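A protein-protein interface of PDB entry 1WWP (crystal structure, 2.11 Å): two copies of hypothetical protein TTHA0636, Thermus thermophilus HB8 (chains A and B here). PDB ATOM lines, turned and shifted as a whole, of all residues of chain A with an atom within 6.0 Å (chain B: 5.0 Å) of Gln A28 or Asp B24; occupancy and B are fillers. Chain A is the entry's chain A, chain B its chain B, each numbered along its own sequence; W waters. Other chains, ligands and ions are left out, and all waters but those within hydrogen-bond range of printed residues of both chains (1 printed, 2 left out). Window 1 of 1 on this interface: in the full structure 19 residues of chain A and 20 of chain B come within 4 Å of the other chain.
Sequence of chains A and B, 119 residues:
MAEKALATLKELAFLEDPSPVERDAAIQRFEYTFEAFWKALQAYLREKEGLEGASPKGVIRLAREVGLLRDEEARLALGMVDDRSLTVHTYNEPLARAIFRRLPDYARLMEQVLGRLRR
Of the 13 printed residues of chain B, 9 touch a printed residue of chain A. Along chain B the printed residues that touch a printed residue of chain A span positions 20 to 90. Hydrophobic or aromatic side chains of chain A within 4 Å of the printed part of chain B: Ala A25, Ile A27 and Tyr A32. Among the printed residues, Asp or Glu carboxylates within 4 Å of a Lys or Arg side-chain nitrogen of the other chain: Arg A29 with Asp B24.
NE2 of Gln A28 sits at hydrogen-bond distance from OE1 of Gln B28 (3.3 Å). The side-chain carboxylate (OE1) of Glu B31 lies within hydrogen-bond range of the side-chain amide nitrogen (NE2) of Gln A28, at 3.0 Å. The side-chain hydroxyl of Thr B90 lies within hydrogen-bond range of the side-chain amide oxygen of Gln A28, at 3.1 Å. OD1 of Asp B24 is in salt-bridge range of NE of Arg A29 (3.0 Å). OE1 of Gln B28 lies close to OE2 of Glu A31 (3.4 Å). The side-chain carboxylate (OE1) of Glu B31 lies close to the side-chain carboxylate (OE2) of Glu A31.
Water W1 lies within hydrogen-bond range of the side-chain carboxylate of Asp B24 (2.4 Å) and the side-chain hydroxyl of Tyr A32 (2.6 Å).
Gln A28 touches six residues of chain B. Asp B24 touches two residues of chain A. Of the printed residues of chain A, Val B21 touches Ala A25 and Arg A29. Of the printed residues of chain A, Pro B20 touches Arg A29. Of the printed residues of chain B, Arg A29 touches Pro B20, Val B21 and Asp B24. Of the printed residues of chain A, Ile B27 touches Gln A28 (3.5 Å). Of the printed residues of chain B, Asp A24 touches Ala B25 and Gln B28. The nearest printed residue of chain B that does not touch Gln A28 is Ala B25 (5.2 Å). The nearest residue of chain A that does not touch Asp B24 is Tyr A32 (4.1 Å).
Among the printed residues, merely in contact across the chains: Gln A28 with Thr B87 (3.3 Å), Ala A25 with Val B21 (3.4 Å), Asp A24 with Gln B28 (3.4 Å), Gln A28 with Ile B27 (3.5 Å), Gln A28 with Asp B24 (3.5 Å), Arg A29 with Pro B20 (3.7 Å), Tyr A32 with Thr B90 (3.7 Å), Ile A27 with Gln B28 (3.7 Å), Ala A25 with Ala B25 (3.9 Å), Asp A24 with Ala B25 (3.9 Å) and Arg A29 with Val B21 (3.99 Å).
Asp A24 touches Ala B25, but with the chains exchanged Ala A25 does not touch Asp B24 (4.1 Å). Asp A24 touches Gln B28, and with the chains exchanged Gln A28 touches Asp B24. Ala B25 touches its own counterpart, Ala A25. Gln A28 touches Glu B31, and with the chains exchanged Glu A31 touches Gln B28.
The backbone carbonyl oxygen of Thr A8 sits at hydrogen-bond distance from the guanidinium group of Arg A29 (2.9 Å). The side-chain hydroxyl of Thr A8 sits at hydrogen-bond distance from the side-chain hydroxyl of Tyr A32, at 2.9 Å. NE2 of Gln A28 is in hydrogen-bond range of OE2 of Glu A31. The backbone carbonyl oxygen (O) of Arg A29 is in hydrogen-bond range of the side-chain hydroxyl (OG1) of Thr A33, 2.7 Å away. The side-chain carboxylate (OE1) of Glu B31 lies close to the side-chain amide oxygen (OE1) of Gln B28. The backbone carbonyl oxygen of Thr B87 is in hydrogen-bond range of the side-chain hydroxyl of Thr B90, at 2.6 Å.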
ATOM      1  N   THR A   8       3.032 -32.565 -12.911  1.00  0.00           N
ATOM      2  CA  THR A   8       3.401 -31.463 -12.034  1.00  0.00           C
ATOM      3  C   THR A   8       3.616 -30.207 -12.872  1.00  0.00           C
ATOM      4  O   THR A   8       3.327 -29.092 -12.426  1.00  0.00           O
ATOM      5  CB  THR A   8       4.666 -31.803 -11.253  1.00  0.00           C
ATOM      6  OG1 THR A   8       5.755 -31.989 -12.165  1.00  0.00           O
ATOM      7  CG2 THR A   8       4.461 -33.099 -10.483  1.00  0.00           C
ATOM      8  N   ARG A  23       6.139 -19.088 -11.734  1.00  0.00           N
ATOM      9  CA  ARG A  23       6.841 -19.085 -13.003  1.00  0.00           C
ATOM     10  C   ARG A  23       8.212 -19.810 -12.901  1.00  0.00           C
ATOM     11  O   ARG A  23       8.538 -20.654 -13.717  1.00  0.00           O
ATOM     12  CB  ARG A  23       7.038 -17.640 -13.438  1.00  0.00           C
ATOM     13  CG  ARG A  23       7.613 -17.458 -14.825  1.00  0.00           C
ATOM     14  CD  ARG A  23       7.877 -15.985 -15.050  1.00  0.00           C
ATOM     15  NE  ARG A  23       6.729 -15.191 -14.617  1.00  0.00           N
ATOM     16  CZ  ARG A  23       6.806 -13.945 -14.166  1.00  0.00           C
ATOM     17  NH1 ARG A  23       7.983 -13.344 -14.087  1.00  0.00           N
ATOM     18  NH2 ARG A  23       5.706 -13.308 -13.782  1.00  0.00           N
ATOM     19  N   ASP A  24       9.007 -19.465 -11.896  1.00  0.00           N
ATOM     20  CA  ASP A  24      10.306 -20.111 -11.713  1.00  0.00           C
ATOM     21  C   ASP A  24      10.103 -21.612 -11.501  1.00  0.00           C
ATOM     22  O   ASP A  24      10.851 -22.434 -12.032  1.00  0.00           O
ATOM     23  CB  ASP A  24      11.041 -19.458 -10.533  1.00  0.00           C
ATOM     24  CG  ASP A  24      11.521 -18.052 -10.869  1.00  0.00           C
ATOM     25  OD1 ASP A  24      12.024 -17.347  -9.965  1.00  0.00           O
ATOM     26  OD2 ASP A  24      11.392 -17.659 -12.059  1.00  0.00           O
ATOM     27  N   ALA A  25       9.070 -21.959 -10.737  1.00  0.00           N
ATOM     28  CA  ALA A  25       8.728 -23.349 -10.469  1.00  0.00           C
ATOM     29  C   ALA A  25       8.324 -24.076 -11.755  1.00  0.00           C
ATOM     30  O   ALA A  25       8.643 -25.244 -11.948  1.00  0.00           O
ATOM     31  CB  ALA A  25       7.578 -23.418  -9.453  1.00  0.00           C
ATOM     32  N   ALA A  26       7.598 -23.390 -12.627  1.00  0.00           N
ATOM     33  CA  ALA A  26       7.159 -23.991 -13.887  1.00  0.00           C
ATOM     34  C   ALA A  26       8.389 -24.260 -14.752  1.00  0.00           C
ATOM     35  O   ALA A  26       8.448 -25.239 -15.481  1.00  0.00           O
ATOM     36  CB  ALA A  26       6.216 -23.055 -14.618  1.00  0.00           C
ATOM     37  N   ILE A  27       9.376 -23.384 -14.658  1.00  0.00           N
ATOM     38  CA  ILE A  27      10.589 -23.551 -15.450  1.00  0.00           C
ATOM     39  C   ILE A  27      11.385 -24.758 -14.954  1.00  0.00           C
ATOM     40  O   ILE A  27      11.897 -25.548 -15.743  1.00  0.00           O
ATOM     41  CB  ILE A  27      11.432 -22.268 -15.387  1.00  0.00           C
ATOM     42  CG1 ILE A  27      10.698 -21.158 -16.138  1.00  0.00           C
ATOM     43  CG2 ILE A  27      12.819 -22.510 -15.952  1.00  0.00           C
ATOM     44  CD1 ILE A  27      11.318 -19.784 -15.949  1.00  0.00           C
ATOM     45  N   GLN A  28      11.468 -24.902 -13.637  1.00  0.00           N
ATOM     46  CA  GLN A  28      12.162 -26.025 -13.031  1.00  0.00           C
ATOM     47  C   GLN A  28      11.486 -27.332 -13.452  1.00  0.00           C
ATOM     48  O   GLN A  28      12.152 -28.297 -13.832  1.00  0.00           O
ATOM     49  CB  GLN A  28      12.143 -25.887 -11.497  1.00  0.00           C
ATOM     50  CG  GLN A  28      12.557 -27.146 -10.733  1.00  0.00           C
ATOM     51  CD  GLN A  28      14.047 -27.478 -10.846  1.00  0.00           C
ATOM     52  OE1 GLN A  28      14.506 -28.469 -10.276  1.00  0.00           O
ATOM     53  NE2 GLN A  28      14.802 -26.654 -11.574  1.00  0.00           N
ATOM     54  N   ARG A  29      10.162 -27.369 -13.400  1.00  0.00           N
ATOM     55  CA  ARG A  29       9.433 -28.582 -13.773  1.00  0.00           C
ATOM     56  C   ARG A  29       9.579 -28.891 -15.243  1.00  0.00           C
ATOM     57  O   ARG A  29       9.634 -30.049 -15.644  1.00  0.00           O
ATOM     58  CB  ARG A  29       7.954 -28.440 -13.400  1.00  0.00           C
ATOM     59  CG  ARG A  29       7.758 -28.306 -11.898  1.00  0.00           C
ATOM     60  CD  ARG A  29       6.286 -28.135 -11.467  1.00  0.00           C
ATOM     61  NE  ARG A  29       6.245 -28.148 -10.007  1.00  0.00           N
ATOM     62  CZ  ARG A  29       5.152 -28.061  -9.253  1.00  0.00           C
ATOM     63  NH1 ARG A  29       3.946 -27.953  -9.804  1.00  0.00           N
ATOM     64  NH2 ARG A  29       5.279 -28.074  -7.934  1.00  0.00           N
ATOM     65  N   PHE A  30       9.615 -27.854 -16.064  1.00  0.00           N
ATOM     66  CA  PHE A  30       9.813 -28.072 -17.487  1.00  0.00           C
ATOM     67  C   PHE A  30      11.170 -28.788 -17.667  1.00  0.00           C
ATOM     68  O   PHE A  30      11.306 -29.722 -18.464  1.00  0.00           O
ATOM     69  CB  PHE A  30       9.823 -26.719 -18.207  1.00  0.00           C
ATOM     70  CG  PHE A  30      10.456 -26.763 -19.570  1.00  0.00           C
ATOM     71  CD1 PHE A  30       9.939 -27.576 -20.568  1.00  0.00           C
ATOM     72  CD2 PHE A  30      11.592 -25.999 -19.844  1.00  0.00           C
ATOM     73  CE1 PHE A  30      10.549 -27.635 -21.829  1.00  0.00           C
ATOM     74  CE2 PHE A  30      12.214 -26.052 -21.114  1.00  0.00           C
ATOM     75  CZ  PHE A  30      11.691 -26.870 -22.099  1.00  0.00           C
ATOM     76  N   GLU A  31      12.165 -28.346 -16.908  1.00  0.00           N
ATOM     77  CA  GLU A  31      13.495 -28.938 -17.002  1.00  0.00           C
ATOM     78  C   GLU A  31      13.474 -30.436 -16.770  1.00  0.00           C
ATOM     79  O   GLU A  31      13.859 -31.207 -17.654  1.00  0.00           O
ATOM     80  CB  GLU A  31      14.443 -28.278 -16.001  1.00  0.00           C
ATOM     81  CG  GLU A  31      14.869 -26.861 -16.380  1.00  0.00           C
ATOM     82  CD  GLU A  31      15.930 -26.305 -15.438  1.00  0.00           C
ATOM     83  OE1 GLU A  31      16.621 -25.337 -15.814  1.00  0.00           O
ATOM     84  OE2 GLU A  31      16.083 -26.833 -14.317  1.00  0.00           O
ATOM     85  N   TYR A  32      13.008 -30.870 -15.599  1.00  0.00           N
ATOM     86  CA  TYR A  32      13.007 -32.299 -15.348  1.00  0.00           C
ATOM     87  C   TYR A  32      12.005 -33.088 -16.170  1.00  0.00           C
ATOM     88  O   TYR A  32      12.170 -34.290 -16.354  1.00  0.00           O
ATOM     89  CB  TYR A  32      12.886 -32.608 -13.843  1.00  0.00           C
ATOM     90  CG  TYR A  32      11.610 -32.236 -13.120  1.00  0.00           C
ATOM     91  CD1 TYR A  32      10.413 -32.891 -13.389  1.00  0.00           C
ATOM     92  CD2 TYR A  32      11.640 -31.313 -12.062  1.00  0.00           C
ATOM     93  CE1 TYR A  32       9.264 -32.647 -12.607  1.00  0.00           C
ATOM     94  CE2 TYR A  32      10.510 -31.063 -11.279  1.00  0.00           C
ATOM     95  CZ  TYR A  32       9.327 -31.736 -11.550  1.00  0.00           C
ATOM     96  OH  TYR A  32       8.232 -31.515 -10.740  1.00  0.00           O
ATOM     97  N   THR A  33      10.980 -32.420 -16.688  1.00  0.00           N
ATOM     98  CA  THR A  33      10.017 -33.107 -17.528  1.00  0.00           C
ATOM     99  C   THR A  33      10.649 -33.341 -18.897  1.00  0.00           C
ATOM    100  O   THR A  33      10.454 -34.379 -19.534  1.00  0.00           O
ATOM    101  CB  THR A  33       8.733 -32.267 -17.726  1.00  0.00           C
ATOM    102  OG1 THR A  33       8.055 -32.128 -16.471  1.00  0.00           O
ATOM    103  CG2 THR A  33       7.819 -32.935 -18.761  1.00  0.00           C
ATOM    104  N   PRO B  20       5.296 -26.966  -2.357  1.00  0.00           N
ATOM    105  CA  PRO B  20       6.012 -27.648  -3.441  1.00  0.00           C
ATOM    106  C   PRO B  20       6.410 -26.659  -4.559  1.00  0.00           C
ATOM    107  O   PRO B  20       7.429 -26.846  -5.228  1.00  0.00           O
ATOM    108  CB  PRO B  20       4.999 -28.692  -3.907  1.00  0.00           C
ATOM    109  CG  PRO B  20       4.328 -29.076  -2.613  1.00  0.00           C
ATOM    110  CD  PRO B  20       4.091 -27.722  -1.962  1.00  0.00           C
ATOM    111  N   VAL B  21       5.607 -25.616  -4.758  1.00  0.00           N
ATOM    112  CA  VAL B  21       5.905 -24.612  -5.779  1.00  0.00           C
ATOM    113  C   VAL B  21       7.059 -23.726  -5.315  1.00  0.00           C
ATOM    114  O   VAL B  21       7.930 -23.367  -6.105  1.00  0.00           O
ATOM    115  CB  VAL B  21       4.662 -23.736  -6.113  1.00  0.00           C
ATOM    116  CG1 VAL B  21       5.076 -22.453  -6.835  1.00  0.00           C
ATOM    117  CG2 VAL B  21       3.725 -24.516  -7.020  1.00  0.00           C
ATOM    118  N   GLU B  22       7.073 -23.390  -4.031  1.00  0.00           N
ATOM    119  CA  GLU B  22       8.140 -22.576  -3.473  1.00  0.00           C
ATOM    120  C   GLU B  22       9.473 -23.339  -3.495  1.00  0.00           C
ATOM    121  O   GLU B  22      10.524 -22.737  -3.679  1.00  0.00           O
ATOM    122  CB  GLU B  22       7.815 -22.188  -2.027  1.00  0.00           C
ATOM    123  CG  GLU B  22       6.624 -21.266  -1.861  1.00  0.00           C
ATOM    124  CD  GLU B  22       6.296 -20.989  -0.397  1.00  0.00           C
ATOM    125  OE1 GLU B  22       6.105 -21.951   0.364  1.00  0.00           O
ATOM    126  OE2 GLU B  22       6.233 -19.807  -0.008  1.00  0.00           O
ATOM    127  N   ARG B  23       9.432 -24.651  -3.276  1.00  0.00           N
ATOM    128  CA  ARG B  23      10.662 -25.465  -3.262  1.00  0.00           C
ATOM    129  C   ARG B  23      11.274 -25.623  -4.665  1.00  0.00           C
ATOM    130  O   ARG B  23      12.487 -25.553  -4.835  1.00  0.00           O
ATOM    131  CB  ARG B  23      10.383 -26.858  -2.682  1.00  0.00           C
ATOM    132  CG  ARG B  23      11.605 -27.760  -2.680  1.00  0.00           C
ATOM    133  CD  ARG B  23      11.242 -29.242  -2.578  1.00  0.00           C
ATOM    134  NE  ARG B  23      10.542 -29.564  -1.336  1.00  0.00           N
ATOM    135  CZ  ARG B  23       9.220 -29.615  -1.212  1.00  0.00           C
ATOM    136  NH1 ARG B  23       8.446 -29.372  -2.259  1.00  0.00           N
ATOM    137  NH2 ARG B  23       8.670 -29.896  -0.036  1.00  0.00           N
ATOM    138  N   ASP B  24      10.430 -25.863  -5.659  1.00  0.00           N
ATOM    139  CA  ASP B  24      10.899 -26.002  -7.023  1.00  0.00           C
ATOM    140  C   ASP B  24      11.415 -24.645  -7.510  1.00  0.00           C
ATOM    141  O   ASP B  24      12.411 -24.585  -8.221  1.00  0.00           O
ATOM    142  CB  ASP B  24       9.783 -26.549  -7.921  1.00  0.00           C
ATOM    143  CG  ASP B  24       9.529 -28.051  -7.688  1.00  0.00           C
ATOM    144  OD1 ASP B  24       8.396 -28.530  -7.970  1.00  0.00           O
ATOM    145  OD2 ASP B  24      10.474 -28.753  -7.232  1.00  0.00           O
ATOM    146  N   ALA B  25      10.772 -23.560  -7.093  1.00  0.00           N
ATOM    147  CA  ALA B  25      11.230 -22.241  -7.495  1.00  0.00           C
ATOM    148  C   ALA B  25      12.594 -21.915  -6.865  1.00  0.00           C
ATOM    149  O   ALA B  25      13.441 -21.279  -7.494  1.00  0.00           O
ATOM    150  CB  ALA B  25      10.207 -21.192  -7.094  1.00  0.00           C
ATOM    151  N   ALA B  26      12.797 -22.341  -5.623  1.00  0.00           N
ATOM    152  CA  ALA B  26      14.047 -22.093  -4.918  1.00  0.00           C
ATOM    153  C   ALA B  26      15.163 -22.871  -5.602  1.00  0.00           C
ATOM    154  O   ALA B  26      16.282 -22.394  -5.670  1.00  0.00           O
ATOM    155  CB  ALA B  26      13.937 -22.518  -3.446  1.00  0.00           C
ATOM    156  N   ILE B  27      14.856 -24.061  -6.107  1.00  0.00           N
ATOM    157  CA  ILE B  27      15.876 -24.840  -6.778  1.00  0.00           C
ATOM    158  C   ILE B  27      16.215 -24.199  -8.121  1.00  0.00           C
ATOM    159  O   ILE B  27      17.379 -24.169  -8.507  1.00  0.00           O
ATOM    160  CB  ILE B  27      15.465 -26.304  -6.955  1.00  0.00           C
ATOM    161  CG1 ILE B  27      15.411 -26.973  -5.572  1.00  0.00           C
ATOM    162  CG2 ILE B  27      16.521 -27.057  -7.795  1.00  0.00           C
ATOM    163  CD1 ILE B  27      14.719 -28.312  -5.587  1.00  0.00           C
ATOM    164  N   GLN B  28      15.209 -23.671  -8.811  1.00  0.00           N
ATOM    165  CA  GLN B  28      15.445 -22.989 -10.092  1.00  0.00           C
ATOM    166  C   GLN B  28      16.353 -21.762  -9.887  1.00  0.00           C
ATOM    167  O   GLN B  28      17.303 -21.553 -10.644  1.00  0.00           O
ATOM    168  CB  GLN B  28      14.105 -22.581 -10.720  1.00  0.00           C
ATOM    169  CG  GLN B  28      14.198 -21.862 -12.063  1.00  0.00           C
ATOM    170  CD  GLN B  28      15.146 -22.539 -13.024  1.00  0.00           C
ATOM    171  OE1 GLN B  28      15.191 -23.767 -13.114  1.00  0.00           O
ATOM    172  NE2 GLN B  28      15.906 -21.737 -13.758  1.00  0.00           N
ATOM    173  N   GLU B  31      19.978 -22.637  -9.369  1.00  0.00           N
ATOM    174  CA  GLU B  31      20.602 -22.929 -10.654  1.00  0.00           C
ATOM    175  C   GLU B  31      21.028 -21.668 -11.383  1.00  0.00           C
ATOM    176  O   GLU B  31      22.174 -21.559 -11.803  1.00  0.00           O
ATOM    177  CB  GLU B  31      19.671 -23.706 -11.572  1.00  0.00           C
ATOM    178  CG  GLU B  31      19.536 -25.197 -11.296  1.00  0.00           C
ATOM    179  CD  GLU B  31      18.651 -25.870 -12.339  1.00  0.00           C
ATOM    180  OE1 GLU B  31      17.463 -25.530 -12.418  1.00  0.00           O
ATOM    181  OE2 GLU B  31      19.142 -26.734 -13.100  1.00  0.00           O
ATOM    182  N   THR B  87      19.946 -31.211 -10.367  1.00  0.00           N
ATOM    183  CA  THR B  87      18.726 -30.422 -10.428  1.00  0.00           C
ATOM    184  C   THR B  87      18.000 -30.765 -11.735  1.00  0.00           C
ATOM    185  O   THR B  87      17.046 -30.094 -12.135  1.00  0.00           O
ATOM    186  CB  THR B  87      19.050 -28.901 -10.374  1.00  0.00           C
ATOM    187  OG1 THR B  87      19.646 -28.579  -9.108  1.00  0.00           O
ATOM    188  CG2 THR B  87      17.795 -28.072 -10.542  1.00  0.00           C
ATOM    189  N   THR B  90      14.864 -33.739 -10.961  1.00  0.00           N
ATOM    190  CA  THR B  90      14.452 -33.297  -9.639  1.00  0.00           C
ATOM    191  C   THR B  90      13.095 -33.691  -9.077  1.00  0.00           C
ATOM    192  O   THR B  90      12.874 -33.503  -7.879  1.00  0.00           O
ATOM    193  CB  THR B  90      14.576 -31.773  -9.507  1.00  0.00           C
ATOM    194  OG1 THR B  90      15.666 -31.313 -10.311  1.00  0.00           O
ATOM    195  CG2 THR B  90      14.862 -31.394  -8.061  1.00  0.00           C
ATOM    196  N   ALA B  96      15.211 -33.287  -4.504  1.00  0.00           N
ATOM    197  CA  ALA B  96      14.826 -31.890  -4.459  1.00  0.00           C
ATOM    198  C   ALA B  96      14.896 -31.419  -3.008  1.00  0.00           C
ATOM    199  O   ALA B  96      15.431 -30.340  -2.715  1.00  0.00           O
ATOM    200  CB  ALA B  96      13.416 -31.708  -5.008  1.00  0.00           C
HETATM  201  O   HOH W   1       7.948 -30.896  -8.212  1.00  0.00           O
